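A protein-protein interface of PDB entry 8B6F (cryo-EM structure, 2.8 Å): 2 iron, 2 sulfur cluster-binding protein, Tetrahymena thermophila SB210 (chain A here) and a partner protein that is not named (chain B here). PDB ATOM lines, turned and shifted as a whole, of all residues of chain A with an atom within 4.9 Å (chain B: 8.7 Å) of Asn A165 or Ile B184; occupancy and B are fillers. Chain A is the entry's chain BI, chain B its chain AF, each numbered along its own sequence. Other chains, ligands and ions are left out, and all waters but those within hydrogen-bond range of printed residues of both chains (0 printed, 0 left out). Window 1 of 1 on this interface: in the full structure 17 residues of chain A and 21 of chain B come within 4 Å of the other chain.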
ATOM      1  N   ARG A  50     -22.246  21.237 -15.218  1.00  0.00           N
ATOM      2  CA  ARG A  50     -21.036  21.655 -15.916  1.00  0.00           C
ATOM      3  C   ARG A  50     -20.444  20.539 -16.764  1.00  0.00           C
ATOM      4  O   ARG A  50     -19.681  20.821 -17.691  1.00  0.00           O
ATOM      5  CB  ARG A  50     -19.994  22.143 -14.909  1.00  0.00           C
ATOM      6  CG  ARG A  50     -19.583  21.085 -13.902  1.00  0.00           C
ATOM      7  CD  ARG A  50     -18.792  21.672 -12.750  1.00  0.00           C
ATOM      8  NE  ARG A  50     -18.465  20.655 -11.759  1.00  0.00           N
ATOM      9  CZ  ARG A  50     -17.836  20.892 -10.616  1.00  0.00           C
ATOM     10  NH1 ARG A  50     -17.447  22.110 -10.281  1.00  0.00           N
ATOM     11  NH2 ARG A  50     -17.594  19.881  -9.788  1.00  0.00           N
ATOM     12  N   VAL A  78     -19.634  28.462  -7.056  1.00  0.00           N
ATOM     13  CA  VAL A  78     -18.672  28.757  -6.002  1.00  0.00           C
ATOM     14  C   VAL A  78     -19.312  29.557  -4.878  1.00  0.00           C
ATOM     15  O   VAL A  78     -19.166  29.219  -3.701  1.00  0.00           O
ATOM     16  CB  VAL A  78     -17.459  29.498  -6.601  1.00  0.00           C
ATOM     17  CG1 VAL A  78     -16.447  29.844  -5.520  1.00  0.00           C
ATOM     18  CG2 VAL A  78     -16.814  28.662  -7.689  1.00  0.00           C
ATOM     19  N   GLN A 162     -19.120  26.251 -15.102  1.00  0.00           N
ATOM     20  CA  GLN A 162     -18.254  26.492 -13.957  1.00  0.00           C
ATOM     21  C   GLN A 162     -18.022  27.984 -13.764  1.00  0.00           C
ATOM     22  O   GLN A 162     -17.769  28.721 -14.721  1.00  0.00           O
ATOM     23  CB  GLN A 162     -16.918  25.775 -14.136  1.00  0.00           C
ATOM     24  CG  GLN A 162     -16.001  25.877 -12.931  1.00  0.00           C
ATOM     25  CD  GLN A 162     -16.605  25.262 -11.690  1.00  0.00           C
ATOM     26  OE1 GLN A 162     -17.372  24.307 -11.774  1.00  0.00           O
ATOM     27  NE2 GLN A 162     -16.268  25.810 -10.529  1.00  0.00           N
ATOM     28  N   ASN A 163     -18.116  28.430 -12.515  1.00  0.00           N
ATOM     29  CA  ASN A 163     -17.876  29.816 -12.153  1.00  0.00           C
ATOM     30  C   ASN A 163     -16.426  30.020 -11.740  1.00  0.00           C
ATOM     31  O   ASN A 163     -15.745  29.077 -11.327  1.00  0.00           O
ATOM     32  CB  ASN A 163     -18.801  30.224 -11.013  1.00  0.00           C
ATOM     33  CG  ASN A 163     -20.252  30.260 -11.429  1.00  0.00           C
ATOM     34  OD1 ASN A 163     -20.572  30.554 -12.577  1.00  0.00           O
ATOM     35  ND2 ASN A 163     -21.140  29.951 -10.496  1.00  0.00           N
ATOM     36  N   PRO A 164     -15.919  31.245 -11.843  1.00  0.00           N
ATOM     37  CA  PRO A 164     -14.519  31.497 -11.489  1.00  0.00           C
ATOM     38  C   PRO A 164     -14.291  31.490  -9.985  1.00  0.00           C
ATOM     39  O   PRO A 164     -15.209  31.665  -9.182  1.00  0.00           O
ATOM     40  CB  PRO A 164     -14.249  32.882 -12.084  1.00  0.00           C
ATOM     41  CG  PRO A 164     -15.575  33.541 -12.092  1.00  0.00           C
ATOM     42  CD  PRO A 164     -16.583  32.459 -12.350  1.00  0.00           C
ATOM     43  N   ASN A 165     -13.031  31.282  -9.613  1.00  0.00           N
ATOM     44  CA  ASN A 165     -12.590  31.355  -8.226  1.00  0.00           C
ATOM     45  C   ASN A 165     -11.922  32.706  -7.996  1.00  0.00           C
ATOM     46  O   ASN A 165     -10.978  33.065  -8.707  1.00  0.00           O
ATOM     47  CB  ASN A 165     -11.624  30.218  -7.895  1.00  0.00           C
ATOM     48  CG  ASN A 165     -12.273  28.854  -8.005  1.00  0.00           C
ATOM     49  OD1 ASN A 165     -12.265  28.235  -9.069  1.00  0.00           O
ATOM     50  ND2 ASN A 165     -12.841  28.379  -6.904  1.00  0.00           N
ATOM     51  N   SER A 166     -12.410  33.445  -7.001  1.00  0.00           N
ATOM     52  CA  SER A 166     -11.982  34.827  -6.822  1.00  0.00           C
ATOM     53  C   SER A 166     -10.653  34.917  -6.081  1.00  0.00           C
ATOM     54  O   SER A 166      -9.663  35.423  -6.618  1.00  0.00           O
ATOM     55  CB  SER A 166     -13.063  35.613  -6.074  1.00  0.00           C
ATOM     56  OG  SER A 166     -14.278  35.631  -6.802  1.00  0.00           O
ATOM     57  N   VAL A 167     -10.612  34.426  -4.844  1.00  0.00           N
ATOM     58  CA  VAL A 167      -9.484  34.685  -3.957  1.00  0.00           C
ATOM     59  C   VAL A 167      -8.859  33.388  -3.466  1.00  0.00           C
ATOM     60  O   VAL A 167      -9.297  32.289  -3.825  1.00  0.00           O
ATOM     61  CB  VAL A 167      -9.913  35.558  -2.763  1.00  0.00           C
ATOM     62  CG1 VAL A 167     -10.212  36.967  -3.222  1.00  0.00           C
ATOM     63  CG2 VAL A 167     -11.124  34.955  -2.068  1.00  0.00           C
ATOM     64  N   ASP A 170     -10.985  30.659  -1.477  1.00  0.00           N
ATOM     65  CA  ASP A 170     -11.863  29.720  -2.166  1.00  0.00           C
ATOM     66  C   ASP A 170     -11.328  28.299  -2.091  1.00  0.00           C
ATOM     67  O   ASP A 170     -12.110  27.345  -2.007  1.00  0.00           O
ATOM     68  CB  ASP A 170     -12.038  30.138  -3.625  1.00  0.00           C
ATOM     69  CG  ASP A 170     -12.937  31.344  -3.784  1.00  0.00           C
ATOM     70  OD1 ASP A 170     -13.960  31.419  -3.076  1.00  0.00           O
ATOM     71  OD2 ASP A 170     -12.621  32.217  -4.617  1.00  0.00           O
ATOM     72  N   ASN B 174     -10.649  20.563   2.281  1.00  0.00           N
ATOM     73  CA  ASN B 174     -11.878  21.198   2.725  1.00  0.00           C
ATOM     74  C   ASN B 174     -13.030  20.197   2.690  1.00  0.00           C
ATOM     75  O   ASN B 174     -12.857  19.016   2.384  1.00  0.00           O
ATOM     76  CB  ASN B 174     -12.179  22.426   1.868  1.00  0.00           C
ATOM     77  CG  ASN B 174     -12.256  22.102   0.392  1.00  0.00           C
ATOM     78  OD1 ASN B 174     -12.310  20.938   0.002  1.00  0.00           O
ATOM     79  ND2 ASN B 174     -12.265  23.135  -0.439  1.00  0.00           N
ATOM     80  N   ASN B 176     -15.632  20.353   0.674  1.00  0.00           N
ATOM     81  CA  ASN B 176     -16.288  20.363  -0.630  1.00  0.00           C
ATOM     82  C   ASN B 176     -15.968  19.056  -1.345  1.00  0.00           C
ATOM     83  O   ASN B 176     -14.816  18.805  -1.711  1.00  0.00           O
ATOM     84  CB  ASN B 176     -15.830  21.564  -1.451  1.00  0.00           C
ATOM     85  CG  ASN B 176     -16.421  21.572  -2.846  1.00  0.00           C
ATOM     86  OD1 ASN B 176     -17.501  22.112  -3.072  1.00  0.00           O
ATOM     87  ND2 ASN B 176     -15.710  20.972  -3.791  1.00  0.00           N
ATOM     88  N   LYS B 178     -17.578  18.067  -4.218  1.00  0.00           N
ATOM     89  CA  LYS B 178     -18.227  18.165  -5.518  1.00  0.00           C
ATOM     90  C   LYS B 178     -17.253  18.229  -6.686  1.00  0.00           C
ATOM     91  O   LYS B 178     -17.670  18.000  -7.826  1.00  0.00           O
ATOM     92  CB  LYS B 178     -19.133  19.401  -5.560  1.00  0.00           C
ATOM     93  CG  LYS B 178     -20.275  19.359  -4.556  1.00  0.00           C
ATOM     94  CD  LYS B 178     -21.112  20.626  -4.594  1.00  0.00           C
ATOM     95  CE  LYS B 178     -20.360  21.816  -4.024  1.00  0.00           C
ATOM     96  NZ  LYS B 178     -21.193  23.050  -4.036  1.00  0.00           N
ATOM     97  N   ASP B 179     -15.979  18.527  -6.437  1.00  0.00           N
ATOM     98  CA  ASP B 179     -14.998  18.742  -7.494  1.00  0.00           C
ATOM     99  C   ASP B 179     -13.982  17.606  -7.580  1.00  0.00           C
ATOM    100  O   ASP B 179     -12.854  17.811  -8.031  1.00  0.00           O
ATOM    101  CB  ASP B 179     -14.280  20.072  -7.280  1.00  0.00           C
ATOM    102  CG  ASP B 179     -15.234  21.245  -7.228  1.00  0.00           C
ATOM    103  OD1 ASP B 179     -16.434  21.048  -7.507  1.00  0.00           O
ATOM    104  OD2 ASP B 179     -14.787  22.363  -6.901  1.00  0.00           O
ATOM    105  N   ASN B 180     -14.368  16.401  -7.158  1.00  0.00           N
ATOM    106  CA  ASN B 180     -13.431  15.284  -7.180  1.00  0.00           C
ATOM    107  C   ASN B 180     -13.023  14.933  -8.604  1.00  0.00           C
ATOM    108  O   ASN B 180     -11.857  14.614  -8.861  1.00  0.00           O
ATOM    109  CB  ASN B 180     -14.044  14.068  -6.485  1.00  0.00           C
ATOM    110  CG  ASN B 180     -14.117  14.230  -4.982  1.00  0.00           C
ATOM    111  OD1 ASN B 180     -13.348  14.983  -4.389  1.00  0.00           O
ATOM    112  ND2 ASN B 180     -15.043  13.516  -4.355  1.00  0.00           N
ATOM    113  N   TYR B 181     -13.967  14.981  -9.541  1.00  0.00           N
ATOM    114  CA  TYR B 181     -13.738  14.546 -10.912  1.00  0.00           C
ATOM    115  C   TYR B 181     -13.975  15.682 -11.902  1.00  0.00           C
ATOM    116  O   TYR B 181     -14.461  15.460 -13.012  1.00  0.00           O
ATOM    117  CB  TYR B 181     -14.626  13.347 -11.243  1.00  0.00           C
ATOM    118  CG  TYR B 181     -14.613  12.287 -10.169  1.00  0.00           C
ATOM    119  CD1 TYR B 181     -13.508  11.467  -9.988  1.00  0.00           C
ATOM    120  CD2 TYR B 181     -15.705  12.111  -9.333  1.00  0.00           C
ATOM    121  CE1 TYR B 181     -13.493  10.500  -9.002  1.00  0.00           C
ATOM    122  CE2 TYR B 181     -15.699  11.148  -8.346  1.00  0.00           C
ATOM    123  CZ  TYR B 181     -14.591  10.345  -8.185  1.00  0.00           C
ATOM    124  OH  TYR B 181     -14.585   9.385  -7.202  1.00  0.00           O
ATOM    125  N   PHE B 182     -13.637  16.905 -11.507  1.00  0.00           N
ATOM    126  CA  PHE B 182     -13.726  18.063 -12.382  1.00  0.00           C
ATOM    127  C   PHE B 182     -12.532  18.968 -12.121  1.00  0.00           C
ATOM    128  O   PHE B 182     -12.027  19.044 -10.999  1.00  0.00           O
ATOM    129  CB  PHE B 182     -15.035  18.834 -12.169  1.00  0.00           C
ATOM    130  CG  PHE B 182     -15.328  19.837 -13.245  1.00  0.00           C
ATOM    131  CD1 PHE B 182     -15.958  19.448 -14.417  1.00  0.00           C
ATOM    132  CD2 PHE B 182     -14.987  21.167 -13.085  1.00  0.00           C
ATOM    133  CE1 PHE B 182     -16.233  20.365 -15.409  1.00  0.00           C
ATOM    134  CE2 PHE B 182     -15.260  22.092 -14.075  1.00  0.00           C
ATOM    135  CZ  PHE B 182     -15.884  21.689 -15.238  1.00  0.00           C
ATOM    136  N   SER B 183     -12.083  19.649 -13.171  1.00  0.00           N
ATOM    137  CA  SER B 183     -10.916  20.518 -13.092  1.00  0.00           C
ATOM    138  C   SER B 183     -11.356  21.923 -12.704  1.00  0.00           C
ATOM    139  O   SER B 183     -12.168  22.539 -13.400  1.00  0.00           O
ATOM    140  CB  SER B 183     -10.172  20.545 -14.424  1.00  0.00           C
ATOM    141  OG  SER B 183      -9.707  19.255 -14.773  1.00  0.00           O
ATOM    142  N   ILE B 184     -10.818  22.424 -11.595  1.00  0.00           N
ATOM    143  CA  ILE B 184     -11.067  23.782 -11.130  1.00  0.00           C
ATOM    144  C   ILE B 184      -9.773  24.564 -11.281  1.00  0.00           C
ATOM    145  O   ILE B 184      -8.713  24.120 -10.822  1.00  0.00           O
ATOM    146  CB  ILE B 184     -11.553  23.802  -9.671  1.00  0.00           C
ATOM    147  CG1 ILE B 184     -12.736  22.850  -9.481  1.00  0.00           C
ATOM    148  CG2 ILE B 184     -11.932  25.215  -9.256  1.00  0.00           C
ATOM    149  CD1 ILE B 184     -13.929  23.153 -10.359  1.00  0.00           C
ATOM    150  N   PHE B 185      -9.856  25.725 -11.920  1.00  0.00           N
ATOM    151  CA  PHE B 185      -8.687  26.530 -12.240  1.00  0.00           C
ATOM    152  C   PHE B 185      -8.614  27.715 -11.287  1.00  0.00           C
ATOM    153  O   PHE B 185      -9.568  28.491 -11.177  1.00  0.00           O
ATOM    154  CB  PHE B 185      -8.742  27.004 -13.689  1.00  0.00           C
ATOM    155  CG  PHE B 185      -9.008  25.907 -14.671  1.00  0.00           C
ATOM    156  CD1 PHE B 185      -8.025  24.983 -14.980  1.00  0.00           C
ATOM    157  CD2 PHE B 185     -10.241  25.801 -15.289  1.00  0.00           C
ATOM    158  CE1 PHE B 185      -8.270  23.971 -15.884  1.00  0.00           C
ATOM    159  CE2 PHE B 185     -10.491  24.792 -16.191  1.00  0.00           C
ATOM    160  CZ  PHE B 185      -9.505  23.877 -16.491  1.00  0.00           C
ATOM    161  N   SER B 186      -7.480  27.850 -10.604  1.00  0.00           N
ATOM    162  CA  SER B 186      -7.213  28.964  -9.704  1.00  0.00           C
ATOM    163  C   SER B 186      -5.889  29.591 -10.112  1.00  0.00           C
ATOM    164  O   SER B 186      -4.865  28.904 -10.152  1.00  0.00           O
ATOM    165  CB  SER B 186      -7.166  28.496  -8.247  1.00  0.00           C
ATOM    166  OG  SER B 186      -6.887  29.574  -7.373  1.00  0.00           O
ATOM    167  N   LYS B 187      -5.910  30.889 -10.410  1.00  0.00           N
ATOM    168  CA  LYS B 187      -4.744  31.593 -10.925  1.00  0.00           C
ATOM    169  C   LYS B 187      -4.059  32.458  -9.876  1.00  0.00           C
ATOM    170  O   LYS B 187      -3.147  33.216 -10.217  1.00  0.00           O
ATOM    171  CB  LYS B 187      -5.130  32.467 -12.119  1.00  0.00           C
ATOM    172  CG  LYS B 187      -5.323  31.715 -13.418  1.00  0.00           C
ATOM    173  CD  LYS B 187      -6.631  30.955 -13.455  1.00  0.00           C
ATOM    174  CE  LYS B 187      -6.834  30.312 -14.815  1.00  0.00           C
ATOM    175  NZ  LYS B 187      -8.231  29.855 -14.988  1.00  0.00           N
ATOM    176  N   ASN B 188      -4.474  32.366  -8.614  1.00  0.00           N
ATOM    177  CA  ASN B 188      -3.935  33.264  -7.598  1.00  0.00           C
ATOM    178  C   ASN B 188      -2.439  33.052  -7.417  1.00  0.00           C
ATOM    179  O   ASN B 188      -1.675  34.016  -7.314  1.00  0.00           O
ATOM    180  CB  ASN B 188      -4.673  33.065  -6.278  1.00  0.00           C
ATOM    181  CG  ASN B 188      -6.128  33.453  -6.370  1.00  0.00           C
ATOM    182  OD1 ASN B 188      -6.485  34.616  -6.195  1.00  0.00           O
ATOM    183  ND2 ASN B 188      -6.983  32.478  -6.651  1.00  0.00           N
ATOM    184  N   ASN B 191      -0.587  34.578 -10.359  1.00  0.00           N
ATOM    185  CA  ASN B 191      -0.701  36.031 -10.322  1.00  0.00           C
ATOM    186  C   ASN B 191       0.247  36.621  -9.289  1.00  0.00           C
ATOM    187  O   ASN B 191       0.950  37.600  -9.565  1.00  0.00           O
ATOM    188  CB  ASN B 191      -2.142  36.439 -10.017  1.00  0.00           C
ATOM    189  CG  ASN B 191      -3.119  35.960 -11.068  1.00  0.00           C
ATOM    190  OD1 ASN B 191      -2.744  35.697 -12.209  1.00  0.00           O
ATOM    191  ND2 ASN B 191      -4.386  35.850 -10.687  1.00  0.00           N
ATOM    192  N   LYS B 274      -4.782  39.505  -2.782  1.00  0.00           N
ATOM    193  CA  LYS B 274      -5.831  38.530  -3.054  1.00  0.00           C
ATOM    194  C   LYS B 274      -5.279  37.111  -3.040  1.00  0.00           C
ATOM    195  O   LYS B 274      -5.904  36.200  -2.487  1.00  0.00           O
ATOM    196  CB  LYS B 274      -6.487  38.822  -4.405  1.00  0.00           C
ATOM    197  CG  LYS B 274      -7.408  40.031  -4.410  1.00  0.00           C
ATOM    198  CD  LYS B 274      -8.317  40.035  -5.630  1.00  0.00           C
ATOM    199  CE  LYS B 274      -7.525  40.032  -6.928  1.00  0.00           C
ATOM    200  NZ  LYS B 274      -8.413  40.123  -8.121  1.00  0.00           N
ATOM    201  N   LEU B 335     -13.640  42.642  -1.832  1.00  0.00           N
ATOM    202  CA  LEU B 335     -12.876  41.546  -1.256  1.00  0.00           C
ATOM    203  C   LEU B 335     -12.163  41.996   0.011  1.00  0.00           C
ATOM    204  O   LEU B 335     -11.744  43.150   0.135  1.00  0.00           O
ATOM    205  CB  LEU B 335     -11.853  41.002  -2.257  1.00  0.00           C
ATOM    206  CG  LEU B 335     -12.445  40.301  -3.481  1.00  0.00           C
ATOM    207  CD1 LEU B 335     -11.367  40.012  -4.504  1.00  0.00           C
ATOM    208  CD2 LEU B 335     -13.156  39.021  -3.079  1.00  0.00           C
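The backbone carbonyl oxygen (O) of Lys B178 is in hydrogen-bond range of the guanidinium group (NH2) of Arg A50, 2.7 Å away.
The side-chain carboxylate (OD1) of Asp B179 lies within salt-bridge range of the guanidinium group (NH2) of Arg A50 (2.8 Å).
The backbone carbonyl oxygen (O) of Phe B185 sits close to the side-chain amide oxygen (OD1) of Asn A165 (3.4 Å).
O of Ser A166 sits close to OD1 of Asn B188, 3.3 Å away.
Of the 16 printed residues of chain B, 7 touch a printed residue of chain A.
Hydrophobic or aromatic side chains of chain A within 4 Å of the printed part of chain B: Val A167.
Among the printed residues, Asp or Glu carboxylates within 4 Å of a Lys or Arg side-chain nitrogen of the other chain: Arg A50 with Asp B179.
Phe B182 touches Arg A50.
Arg A50 touches Ile B184.
Gln A162 touches Phe B182.
Gln A162 touches Ile B184.
Asn A165 touches Ile B184 (OD1 to CG2, 3.0 Å).
Asn B188 touches Val A167 (ND2 to O, 3.7 Å).
Val A167 touches Leu B335 (CG1 to CD1, 3.5 Å).
The side-chain amide nitrogen (ND2) of Asn B176 lies close to the backbone NH (N) of Lys B178, 3.5 Å away.
ND2 of Asn B188 is in hydrogen-bond range of OG of Ser B186 (3.0 Å).
The guanidinium group (NH1) of Arg A50 sits at hydrogen-bond distance from the side-chain amide oxygen (OE1) of Gln A162, at 2.7 Å.
The backbone NH (N) of Ser A166 is in hydrogen-bond range of the side-chain carboxylate (OD2) of Asp A170, at 2.7 Å.
N of Val A167 lies within hydrogen-bond range of OD2 of Asp A170.
Of the printed residues of chain B, Gln A162 touches Phe B182 (3.8 Å) and Ile B184 (3.5 Å).
Asn A163 touches none of the printed residues of chain B.
Asn A165 touches two residues of chain B.
Ser A166 touches just one residue of chain B: Asn B188 (3.3 Å).
Printed residues of chain A within 4 Å of Lys B178: Arg A50 (2.7 Å).
Of the printed residues of chain A, Phe B182 touches Arg A50 and Gln A162.
Of chain A, only Arg A50, Gln A162 and Asn A165 come within 4 Å of Ile B184.
Of the printed residues of chain A, Phe B185 touches Asn A165.
Lys B274 touches none of the printed residues of chain A.
Of the printed residues of chain A, Leu B335 touches Val A167 (3.5 Å).
The nearest residue of chain B that does not touch Asn A165 is Asn B188 (4.5 Å).
The nearest printed residue of chain A that does not touch Phe B182 is Asn A163 (7.1 Å).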
